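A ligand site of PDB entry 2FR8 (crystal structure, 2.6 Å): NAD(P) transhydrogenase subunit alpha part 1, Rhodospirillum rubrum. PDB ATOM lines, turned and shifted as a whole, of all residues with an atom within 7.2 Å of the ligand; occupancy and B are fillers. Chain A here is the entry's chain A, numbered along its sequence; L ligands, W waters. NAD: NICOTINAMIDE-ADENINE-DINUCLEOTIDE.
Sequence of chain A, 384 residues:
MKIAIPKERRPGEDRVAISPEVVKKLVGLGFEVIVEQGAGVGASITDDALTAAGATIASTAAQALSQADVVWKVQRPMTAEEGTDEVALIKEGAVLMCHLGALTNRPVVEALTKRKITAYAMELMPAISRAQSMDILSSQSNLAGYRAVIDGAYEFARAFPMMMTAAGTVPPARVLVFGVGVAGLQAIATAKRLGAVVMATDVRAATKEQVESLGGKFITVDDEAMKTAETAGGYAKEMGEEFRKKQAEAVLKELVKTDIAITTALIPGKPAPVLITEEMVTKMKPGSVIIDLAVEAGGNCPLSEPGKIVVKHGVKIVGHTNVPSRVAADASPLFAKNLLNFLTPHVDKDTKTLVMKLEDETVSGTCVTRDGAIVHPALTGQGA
N of Val 180 lies within hydrogen-bond range of OD2 of Asp 202. O of Arg 204 is in hydrogen-bond range of OG1 of Thr 207 (2.6 Å). The backbone carbonyl oxygen (O) of Gly 179 lies within hydrogen-bond range of the side-chain hydroxyl (OG1) of Thr 264. O of Thr 201 is in hydrogen-bond range of N of Gly 179. N of Thr 264 is in hydrogen-bond range of O of Phe 178 (3.0 Å).
Water W1 lies within hydrogen-bond range of the backbone NH (N) of Ala 183 (2.6 Å), an oxygen (O1N) of the ligand (2.8 Å) and the backbone NH (N) of Val 182 (2.9 Å).
An oxygen (O3B) of the ligand lies within hydrogen-bond range of the backbone carbonyl oxygen (O) of Val 180 (2.5 Å). An oxygen (O2B) of the ligand lies within hydrogen-bond range of the side-chain carboxylate (OD1) of Asp 202 (2.8 Å). NH2 of Arg 204 lies within hydrogen-bond range of O3B of the ligand (2.9 Å). N of Val 182 lies within hydrogen-bond range of O1N of the ligand (2.9 Å).
Residues that only touch the ligand: Gly 179, Gly 181, Val 203, Thr 264, Ala 265 and Leu 275. Hydrophobic or aromatic side chains that line the ligand: Val 182, Val 203, Ala 265 and Leu 275. Within 4 Å of the ligand: Gly 179, Val 180, Gly 181, Val 182, Asp 202, Val 203, Arg 204, Thr 264, Ala 265 and Leu 275.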
ATOM      1  N   GLN A 132     -15.378  11.519 -27.398  1.00  0.00           N
ATOM      2  CA  GLN A 132     -16.313  12.570 -27.819  1.00  0.00           C
ATOM      3  C   GLN A 132     -17.113  12.148 -29.032  1.00  0.00           C
ATOM      4  O   GLN A 132     -18.255  12.571 -29.208  1.00  0.00           O
ATOM      5  CB  GLN A 132     -15.578  13.875 -28.120  1.00  0.00           C
ATOM      6  CG  GLN A 132     -14.865  14.458 -26.916  1.00  0.00           C
ATOM      7  CD  GLN A 132     -15.754  14.526 -25.680  1.00  0.00           C
ATOM      8  OE1 GLN A 132     -16.611  15.395 -25.574  1.00  0.00           O
ATOM      9  NE2 GLN A 132     -15.557  13.589 -24.760  1.00  0.00           N
ATOM     10  N   ASP A 135     -19.932  10.547 -27.609  1.00  0.00           N
ATOM     11  CA  ASP A 135     -20.715  11.354 -26.677  1.00  0.00           C
ATOM     12  C   ASP A 135     -22.052  11.779 -27.281  1.00  0.00           C
ATOM     13  O   ASP A 135     -22.107  12.570 -28.232  1.00  0.00           O
ATOM     14  CB  ASP A 135     -19.920  12.603 -26.261  1.00  0.00           C
ATOM     15  CG  ASP A 135     -20.450  13.214 -24.977  1.00  0.00           C
ATOM     16  OD1 ASP A 135     -20.327  12.560 -23.930  1.00  0.00           O
ATOM     17  OD2 ASP A 135     -20.963  14.357 -25.023  1.00  0.00           O
ATOM     18  N   LEU A 137     -24.516  13.330 -25.521  1.00  0.00           N
ATOM     19  CA  LEU A 137     -24.948  14.600 -24.953  1.00  0.00           C
ATOM     20  C   LEU A 137     -24.520  15.768 -25.821  1.00  0.00           C
ATOM     21  O   LEU A 137     -25.333  16.621 -26.156  1.00  0.00           O
ATOM     22  CB  LEU A 137     -24.421  14.780 -23.527  1.00  0.00           C
ATOM     23  CG  LEU A 137     -25.097  13.914 -22.462  1.00  0.00           C
ATOM     24  CD1 LEU A 137     -24.399  14.108 -21.121  1.00  0.00           C
ATOM     25  CD2 LEU A 137     -26.592  14.220 -22.329  1.00  0.00           C
ATOM     26  N   SER A 138     -23.233  15.797 -26.186  1.00  0.00           N
ATOM     27  CA  SER A 138     -22.728  16.840 -27.067  1.00  0.00           C
ATOM     28  C   SER A 138     -23.412  16.745 -28.430  1.00  0.00           C
ATOM     29  O   SER A 138     -24.099  17.679 -28.844  1.00  0.00           O
ATOM     30  CB  SER A 138     -21.211  16.740 -27.228  1.00  0.00           C
ATOM     31  OG  SER A 138     -20.829  15.516 -27.828  1.00  0.00           O
ATOM     32  N   SER A 141     -27.089  17.774 -27.901  1.00  0.00           N
ATOM     33  CA  SER A 141     -27.207  19.141 -27.376  1.00  0.00           C
ATOM     34  C   SER A 141     -26.678  20.174 -28.368  1.00  0.00           C
ATOM     35  O   SER A 141     -27.055  21.335 -28.324  1.00  0.00           O
ATOM     36  CB  SER A 141     -26.480  19.307 -26.034  1.00  0.00           C
ATOM     37  OG  SER A 141     -25.083  19.134 -26.188  1.00  0.00           O
ATOM     38  N   VAL A 177     -26.754  34.655 -25.070  1.00  0.00           N
ATOM     39  CA  VAL A 177     -26.691  33.222 -24.836  1.00  0.00           C
ATOM     40  C   VAL A 177     -26.153  32.946 -23.444  1.00  0.00           C
ATOM     41  O   VAL A 177     -25.008  33.285 -23.130  1.00  0.00           O
ATOM     42  CB  VAL A 177     -25.786  32.527 -25.886  1.00  0.00           C
ATOM     43  CG1 VAL A 177     -25.648  31.036 -25.602  1.00  0.00           C
ATOM     44  CG2 VAL A 177     -26.359  32.750 -27.280  1.00  0.00           C
ATOM     45  N   PHE A 178     -26.978  32.323 -22.604  1.00  0.00           N
ATOM     46  CA  PHE A 178     -26.584  31.973 -21.250  1.00  0.00           C
ATOM     47  C   PHE A 178     -25.943  30.594 -21.211  1.00  0.00           C
ATOM     48  O   PHE A 178     -26.562  29.601 -21.604  1.00  0.00           O
ATOM     49  CB  PHE A 178     -27.784  31.981 -20.318  1.00  0.00           C
ATOM     50  CG  PHE A 178     -28.290  33.342 -20.004  1.00  0.00           C
ATOM     51  CD1 PHE A 178     -29.068  34.037 -20.921  1.00  0.00           C
ATOM     52  CD2 PHE A 178     -27.999  33.931 -18.789  1.00  0.00           C
ATOM     53  CE1 PHE A 178     -29.530  35.293 -20.632  1.00  0.00           C
ATOM     54  CE2 PHE A 178     -28.471  35.196 -18.493  1.00  0.00           C
ATOM     55  CZ  PHE A 178     -29.239  35.882 -19.417  1.00  0.00           C
ATOM     56  N   GLY A 179     -24.718  30.548 -20.708  1.00  0.00           N
ATOM     57  CA  GLY A 179     -23.987  29.293 -20.601  1.00  0.00           C
ATOM     58  C   GLY A 179     -23.481  28.885 -21.957  1.00  0.00           C
ATOM     59  O   GLY A 179     -24.225  28.381 -22.797  1.00  0.00           O
ATOM     60  N   VAL A 180     -22.187  29.111 -22.165  1.00  0.00           N
ATOM     61  CA  VAL A 180     -21.508  28.632 -23.355  1.00  0.00           C
ATOM     62  C   VAL A 180     -21.647  27.119 -23.233  1.00  0.00           C
ATOM     63  O   VAL A 180     -22.091  26.624 -22.211  1.00  0.00           O
ATOM     64  CB  VAL A 180     -20.072  29.195 -23.421  1.00  0.00           C
ATOM     65  CG1 VAL A 180     -19.250  28.606 -24.541  1.00  0.00           C
ATOM     66  CG2 VAL A 180     -20.195  30.696 -23.653  1.00  0.00           C
ATOM     67  N   GLY A 181     -21.309  26.380 -24.280  1.00  0.00           N
ATOM     68  CA  GLY A 181     -21.775  25.004 -24.303  1.00  0.00           C
ATOM     69  C   GLY A 181     -21.335  24.314 -25.552  1.00  0.00           C
ATOM     70  O   GLY A 181     -20.656  24.867 -26.368  1.00  0.00           O
ATOM     71  N   VAL A 182     -21.731  23.071 -25.670  1.00  0.00           N
ATOM     72  CA  VAL A 182     -21.914  22.504 -26.977  1.00  0.00           C
ATOM     73  C   VAL A 182     -23.154  23.230 -27.514  1.00  0.00           C
ATOM     74  O   VAL A 182     -23.111  23.824 -28.600  1.00  0.00           O
ATOM     75  CB  VAL A 182     -22.142  20.997 -26.908  1.00  0.00           C
ATOM     76  CG1 VAL A 182     -22.428  20.447 -28.271  1.00  0.00           C
ATOM     77  CG2 VAL A 182     -20.906  20.324 -26.335  1.00  0.00           C
ATOM     78  N   ALA A 183     -24.229  23.194 -26.734  1.00  0.00           N
ATOM     79  CA  ALA A 183     -25.484  23.861 -27.086  1.00  0.00           C
ATOM     80  C   ALA A 183     -25.299  25.368 -27.213  1.00  0.00           C
ATOM     81  O   ALA A 183     -25.650  25.967 -28.234  1.00  0.00           O
ATOM     82  CB  ALA A 183     -26.564  23.552 -26.056  1.00  0.00           C
ATOM     83  N   GLY A 184     -24.764  25.976 -26.159  1.00  0.00           N
ATOM     84  CA  GLY A 184     -24.487  27.412 -26.143  1.00  0.00           C
ATOM     85  C   GLY A 184     -23.625  27.900 -27.291  1.00  0.00           C
ATOM     86  O   GLY A 184     -23.970  28.892 -27.949  1.00  0.00           O
ATOM     87  N   LEU A 185     -22.510  27.215 -27.555  1.00  0.00           N
ATOM     88  CA  LEU A 185     -21.613  27.582 -28.666  1.00  0.00           C
ATOM     89  C   LEU A 185     -22.279  27.434 -30.016  1.00  0.00           C
ATOM     90  O   LEU A 185     -21.970  28.167 -30.956  1.00  0.00           O
ATOM     91  CB  LEU A 185     -20.349  26.720 -28.678  1.00  0.00           C
ATOM     92  CG  LEU A 185     -19.315  27.017 -27.593  1.00  0.00           C
ATOM     93  CD1 LEU A 185     -18.325  25.862 -27.437  1.00  0.00           C
ATOM     94  CD2 LEU A 185     -18.568  28.313 -27.855  1.00  0.00           C
ATOM     95  N   THR A 201     -22.364  34.668 -21.877  1.00  0.00           N
ATOM     96  CA  THR A 201     -21.769  34.590 -20.557  1.00  0.00           C
ATOM     97  C   THR A 201     -21.750  33.149 -20.065  1.00  0.00           C
ATOM     98  O   THR A 201     -22.528  32.306 -20.522  1.00  0.00           O
ATOM     99  CB  THR A 201     -22.510  35.466 -19.517  1.00  0.00           C
ATOM    100  OG1 THR A 201     -21.922  35.292 -18.226  1.00  0.00           O
ATOM    101  CG2 THR A 201     -24.001  35.120 -19.467  1.00  0.00           C
ATOM    102  N   ASP A 202     -20.867  32.910 -19.112  1.00  0.00           N
ATOM    103  CA  ASP A 202     -20.662  31.593 -18.524  1.00  0.00           C
ATOM    104  C   ASP A 202     -19.683  31.743 -17.366  1.00  0.00           C
ATOM    105  O   ASP A 202     -18.822  32.628 -17.407  1.00  0.00           O
ATOM    106  CB  ASP A 202     -20.104  30.610 -19.562  1.00  0.00           C
ATOM    107  CG  ASP A 202     -20.116  29.161 -19.089  1.00  0.00           C
ATOM    108  OD1 ASP A 202     -20.470  28.874 -17.922  1.00  0.00           O
ATOM    109  OD2 ASP A 202     -19.749  28.280 -19.901  1.00  0.00           O
ATOM    110  N   VAL A 203     -19.781  30.866 -16.368  1.00  0.00           N
ATOM    111  CA  VAL A 203     -18.903  30.932 -15.194  1.00  0.00           C
ATOM    112  C   VAL A 203     -17.468  30.418 -15.502  1.00  0.00           C
ATOM    113  O   VAL A 203     -16.541  30.653 -14.731  1.00  0.00           O
ATOM    114  CB  VAL A 203     -19.498  30.191 -13.949  1.00  0.00           C
ATOM    115  CG1 VAL A 203     -18.678  30.454 -12.676  1.00  0.00           C
ATOM    116  CG2 VAL A 203     -20.936  30.664 -13.685  1.00  0.00           C
ATOM    117  N   ARG A 204     -17.292  29.754 -16.650  1.00  0.00           N
ATOM    118  CA  ARG A 204     -15.974  29.220 -17.034  1.00  0.00           C
ATOM    119  C   ARG A 204     -15.110  30.258 -17.785  1.00  0.00           C
ATOM    120  O   ARG A 204     -15.557  30.842 -18.776  1.00  0.00           O
ATOM    121  CB  ARG A 204     -16.128  27.926 -17.844  1.00  0.00           C
ATOM    122  CG  ARG A 204     -16.687  26.765 -17.004  1.00  0.00           C
ATOM    123  CD  ARG A 204     -16.340  25.381 -17.559  1.00  0.00           C
ATOM    124  NE  ARG A 204     -17.233  24.913 -18.622  1.00  0.00           N
ATOM    125  CZ  ARG A 204     -17.019  25.033 -19.943  1.00  0.00           C
ATOM    126  NH1 ARG A 204     -15.936  25.633 -20.419  1.00  0.00           N
ATOM    127  NH2 ARG A 204     -17.922  24.551 -20.792  1.00  0.00           N
ATOM    128  N   THR A 207     -13.874  30.258 -21.628  1.00  0.00           N
ATOM    129  CA  THR A 207     -14.975  30.543 -22.539  1.00  0.00           C
ATOM    130  C   THR A 207     -14.643  31.596 -23.589  1.00  0.00           C
ATOM    131  O   THR A 207     -14.846  31.349 -24.781  1.00  0.00           O
ATOM    132  CB  THR A 207     -16.176  31.030 -21.739  1.00  0.00           C
ATOM    133  OG1 THR A 207     -16.703  29.949 -20.958  1.00  0.00           O
ATOM    134  CG2 THR A 207     -17.235  31.556 -22.646  1.00  0.00           C
ATOM    135  N   THR A 264     -28.865  27.647 -21.626  1.00  0.00           N
ATOM    136  CA  THR A 264     -28.513  26.238 -21.837  1.00  0.00           C
ATOM    137  C   THR A 264     -27.869  25.541 -20.631  1.00  0.00           C
ATOM    138  O   THR A 264     -27.450  24.391 -20.743  1.00  0.00           O
ATOM    139  CB  THR A 264     -27.533  26.082 -23.026  1.00  0.00           C
ATOM    140  OG1 THR A 264     -26.223  26.463 -22.623  1.00  0.00           O
ATOM    141  CG2 THR A 264     -27.970  26.935 -24.213  1.00  0.00           C
ATOM    142  N   ALA A 265     -27.791  26.227 -19.496  1.00  0.00           N
ATOM    143  CA  ALA A 265     -27.048  25.725 -18.329  1.00  0.00           C
ATOM    144  C   ALA A 265     -27.793  24.573 -17.661  1.00  0.00           C
ATOM    145  O   ALA A 265     -28.956  24.714 -17.274  1.00  0.00           O
ATOM    146  CB  ALA A 265     -26.792  26.835 -17.336  1.00  0.00           C
ATOM    147  N   LEU A 266     -27.120  23.431 -17.531  1.00  0.00           N
ATOM    148  CA  LEU A 266     -27.666  22.240 -16.892  1.00  0.00           C
ATOM    149  C   LEU A 266     -26.693  21.742 -15.835  1.00  0.00           C
ATOM    150  O   LEU A 266     -25.486  21.968 -15.946  1.00  0.00           O
ATOM    151  CB  LEU A 266     -27.916  21.143 -17.933  1.00  0.00           C
ATOM    152  CG  LEU A 266     -28.245  19.721 -17.458  1.00  0.00           C
ATOM    153  CD1 LEU A 266     -29.599  19.663 -16.756  1.00  0.00           C
ATOM    154  CD2 LEU A 266     -28.237  18.752 -18.634  1.00  0.00           C
ATOM    155  N   ILE A 267     -27.231  21.076 -14.819  1.00  0.00           N
ATOM    156  CA  ILE A 267     -26.432  20.386 -13.795  1.00  0.00           C
ATOM    157  C   ILE A 267     -26.846  18.911 -13.740  1.00  0.00           C
ATOM    158  O   ILE A 267     -28.037  18.601 -13.739  1.00  0.00           O
ATOM    159  CB  ILE A 267     -26.594  21.041 -12.409  1.00  0.00           C
ATOM    160  CG1 ILE A 267     -26.271  22.538 -12.454  1.00  0.00           C
ATOM    161  CG2 ILE A 267     -25.717  20.335 -11.376  1.00  0.00           C
ATOM    162  CD1 ILE A 267     -24.814  22.896 -12.799  1.00  0.00           C
ATOM    163  N   PRO A 268     -25.849  17.978 -13.718  1.00  0.00           N
ATOM    164  CA  PRO A 268     -26.162  16.551 -13.582  1.00  0.00           C
ATOM    165  C   PRO A 268     -26.777  16.194 -12.221  1.00  0.00           C
ATOM    166  O   PRO A 268     -26.157  16.396 -11.173  1.00  0.00           O
ATOM    167  CB  PRO A 268     -24.789  15.882 -13.745  1.00  0.00           C
ATOM    168  CG  PRO A 268     -23.946  16.887 -14.419  1.00  0.00           C
ATOM    169  CD  PRO A 268     -24.408  18.182 -13.876  1.00  0.00           C
ATOM    170  N   PRO A 273     -29.822  25.745 -12.861  1.00  0.00           N
ATOM    171  CA  PRO A 273     -29.578  27.025 -12.212  1.00  0.00           C
ATOM    172  C   PRO A 273     -30.556  28.087 -12.688  1.00  0.00           C
ATOM    173  O   PRO A 273     -31.019  28.013 -13.822  1.00  0.00           O
ATOM    174  CB  PRO A 273     -28.149  27.370 -12.638  1.00  0.00           C
ATOM    175  CG  PRO A 273     -27.959  26.648 -13.913  1.00  0.00           C
ATOM    176  CD  PRO A 273     -28.766  25.413 -13.826  1.00  0.00           C
ATOM    177  N   VAL A 274     -30.865  29.042 -11.823  1.00  0.00           N
ATOM    178  CA  VAL A 274     -31.784  30.142 -12.149  1.00  0.00           C
ATOM    179  C   VAL A 274     -30.965  31.355 -12.588  1.00  0.00           C
ATOM    180  O   VAL A 274     -30.468  32.112 -11.763  1.00  0.00           O
ATOM    181  CB  VAL A 274     -32.783  30.465 -10.972  1.00  0.00           C
ATOM    182  CG1 VAL A 274     -32.102  30.442  -9.597  1.00  0.00           C
ATOM    183  CG2 VAL A 274     -33.507  31.796 -11.208  1.00  0.00           C
ATOM    184  N   LEU A 275     -30.815  31.501 -13.913  1.00  0.00           N
ATOM    185  CA  LEU A 275     -30.021  32.583 -14.496  1.00  0.00           C
ATOM    186  C   LEU A 275     -30.882  33.797 -14.842  1.00  0.00           C
ATOM    187  O   LEU A 275     -30.375  34.920 -14.909  1.00  0.00           O
ATOM    188  CB  LEU A 275     -29.277  32.117 -15.755  1.00  0.00           C
ATOM    189  CG  LEU A 275     -28.246  30.991 -15.618  1.00  0.00           C
ATOM    190  CD1 LEU A 275     -28.917  29.651 -15.644  1.00  0.00           C
ATOM    191  CD2 LEU A 275     -27.221  31.017 -16.736  1.00  0.00           C
HETATM  192  PA  NAD L   1     -23.030  20.964 -20.265  1.00  0.00           P
HETATM  193  O1A NAD L   1     -24.009  20.747 -21.365  1.00  0.00           O
HETATM  194  O2A NAD L   1     -23.232  19.989 -19.156  1.00  0.00           O
HETATM  195  O5B NAD L   1     -23.162  22.463 -19.692  1.00  0.00           O
HETATM  196  C5B NAD L   1     -23.587  23.532 -20.510  1.00  0.00           C
HETATM  197  C4B NAD L   1     -22.910  24.849 -20.116  1.00  0.00           C
HETATM  198  O4B NAD L   1     -23.587  25.510 -19.065  1.00  0.00           O
HETATM  199  C3B NAD L   1     -21.450  24.749 -19.691  1.00  0.00           C
HETATM  200  O3B NAD L   1     -20.617  25.479 -20.583  1.00  0.00           O
HETATM  201  C2B NAD L   1     -21.413  25.379 -18.309  1.00  0.00           C
HETATM  202  O2B NAD L   1     -20.224  26.106 -18.079  1.00  0.00           O
HETATM  203  C1B NAD L   1     -22.638  26.291 -18.356  1.00  0.00           C
HETATM  204  N9A NAD L   1     -23.119  26.752 -17.039  1.00  0.00           N
HETATM  205  C8A NAD L   1     -23.412  26.006 -15.922  1.00  0.00           C
HETATM  206  N7A NAD L   1     -23.828  26.839 -14.939  1.00  0.00           N
HETATM  207  C5A NAD L   1     -23.814  28.117 -15.392  1.00  0.00           C
HETATM  208  C6A NAD L   1     -24.141  29.365 -14.830  1.00  0.00           C
HETATM  209  N6A NAD L   1     -24.587  29.505 -13.578  1.00  0.00           N
HETATM  210  N1A NAD L   1     -24.018  30.512 -15.586  1.00  0.00           N
HETATM  211  C2A NAD L   1     -23.579  30.438 -16.890  1.00  0.00           C
HETATM  212  N3A NAD L   1     -23.259  29.215 -17.431  1.00  0.00           N
HETATM  213  C4A NAD L   1     -23.378  28.067 -16.713  1.00  0.00           C
HETATM  214  O3  NAD L   1     -21.514  20.880 -20.809  1.00  0.00           O
HETATM  215  PN  NAD L   1     -21.185  20.435 -22.317  1.00  0.00           P
HETATM  216  O1N NAD L   1     -21.766  21.469 -23.205  1.00  0.00           O
HETATM  217  O2N NAD L   1     -21.526  19.005 -22.495  1.00  0.00           O
HETATM  218  O5D NAD L   1     -19.574  20.585 -22.373  1.00  0.00           O
HETATM  219  O   HOH W   1     -24.154  22.643 -24.179  1.00  0.00           O
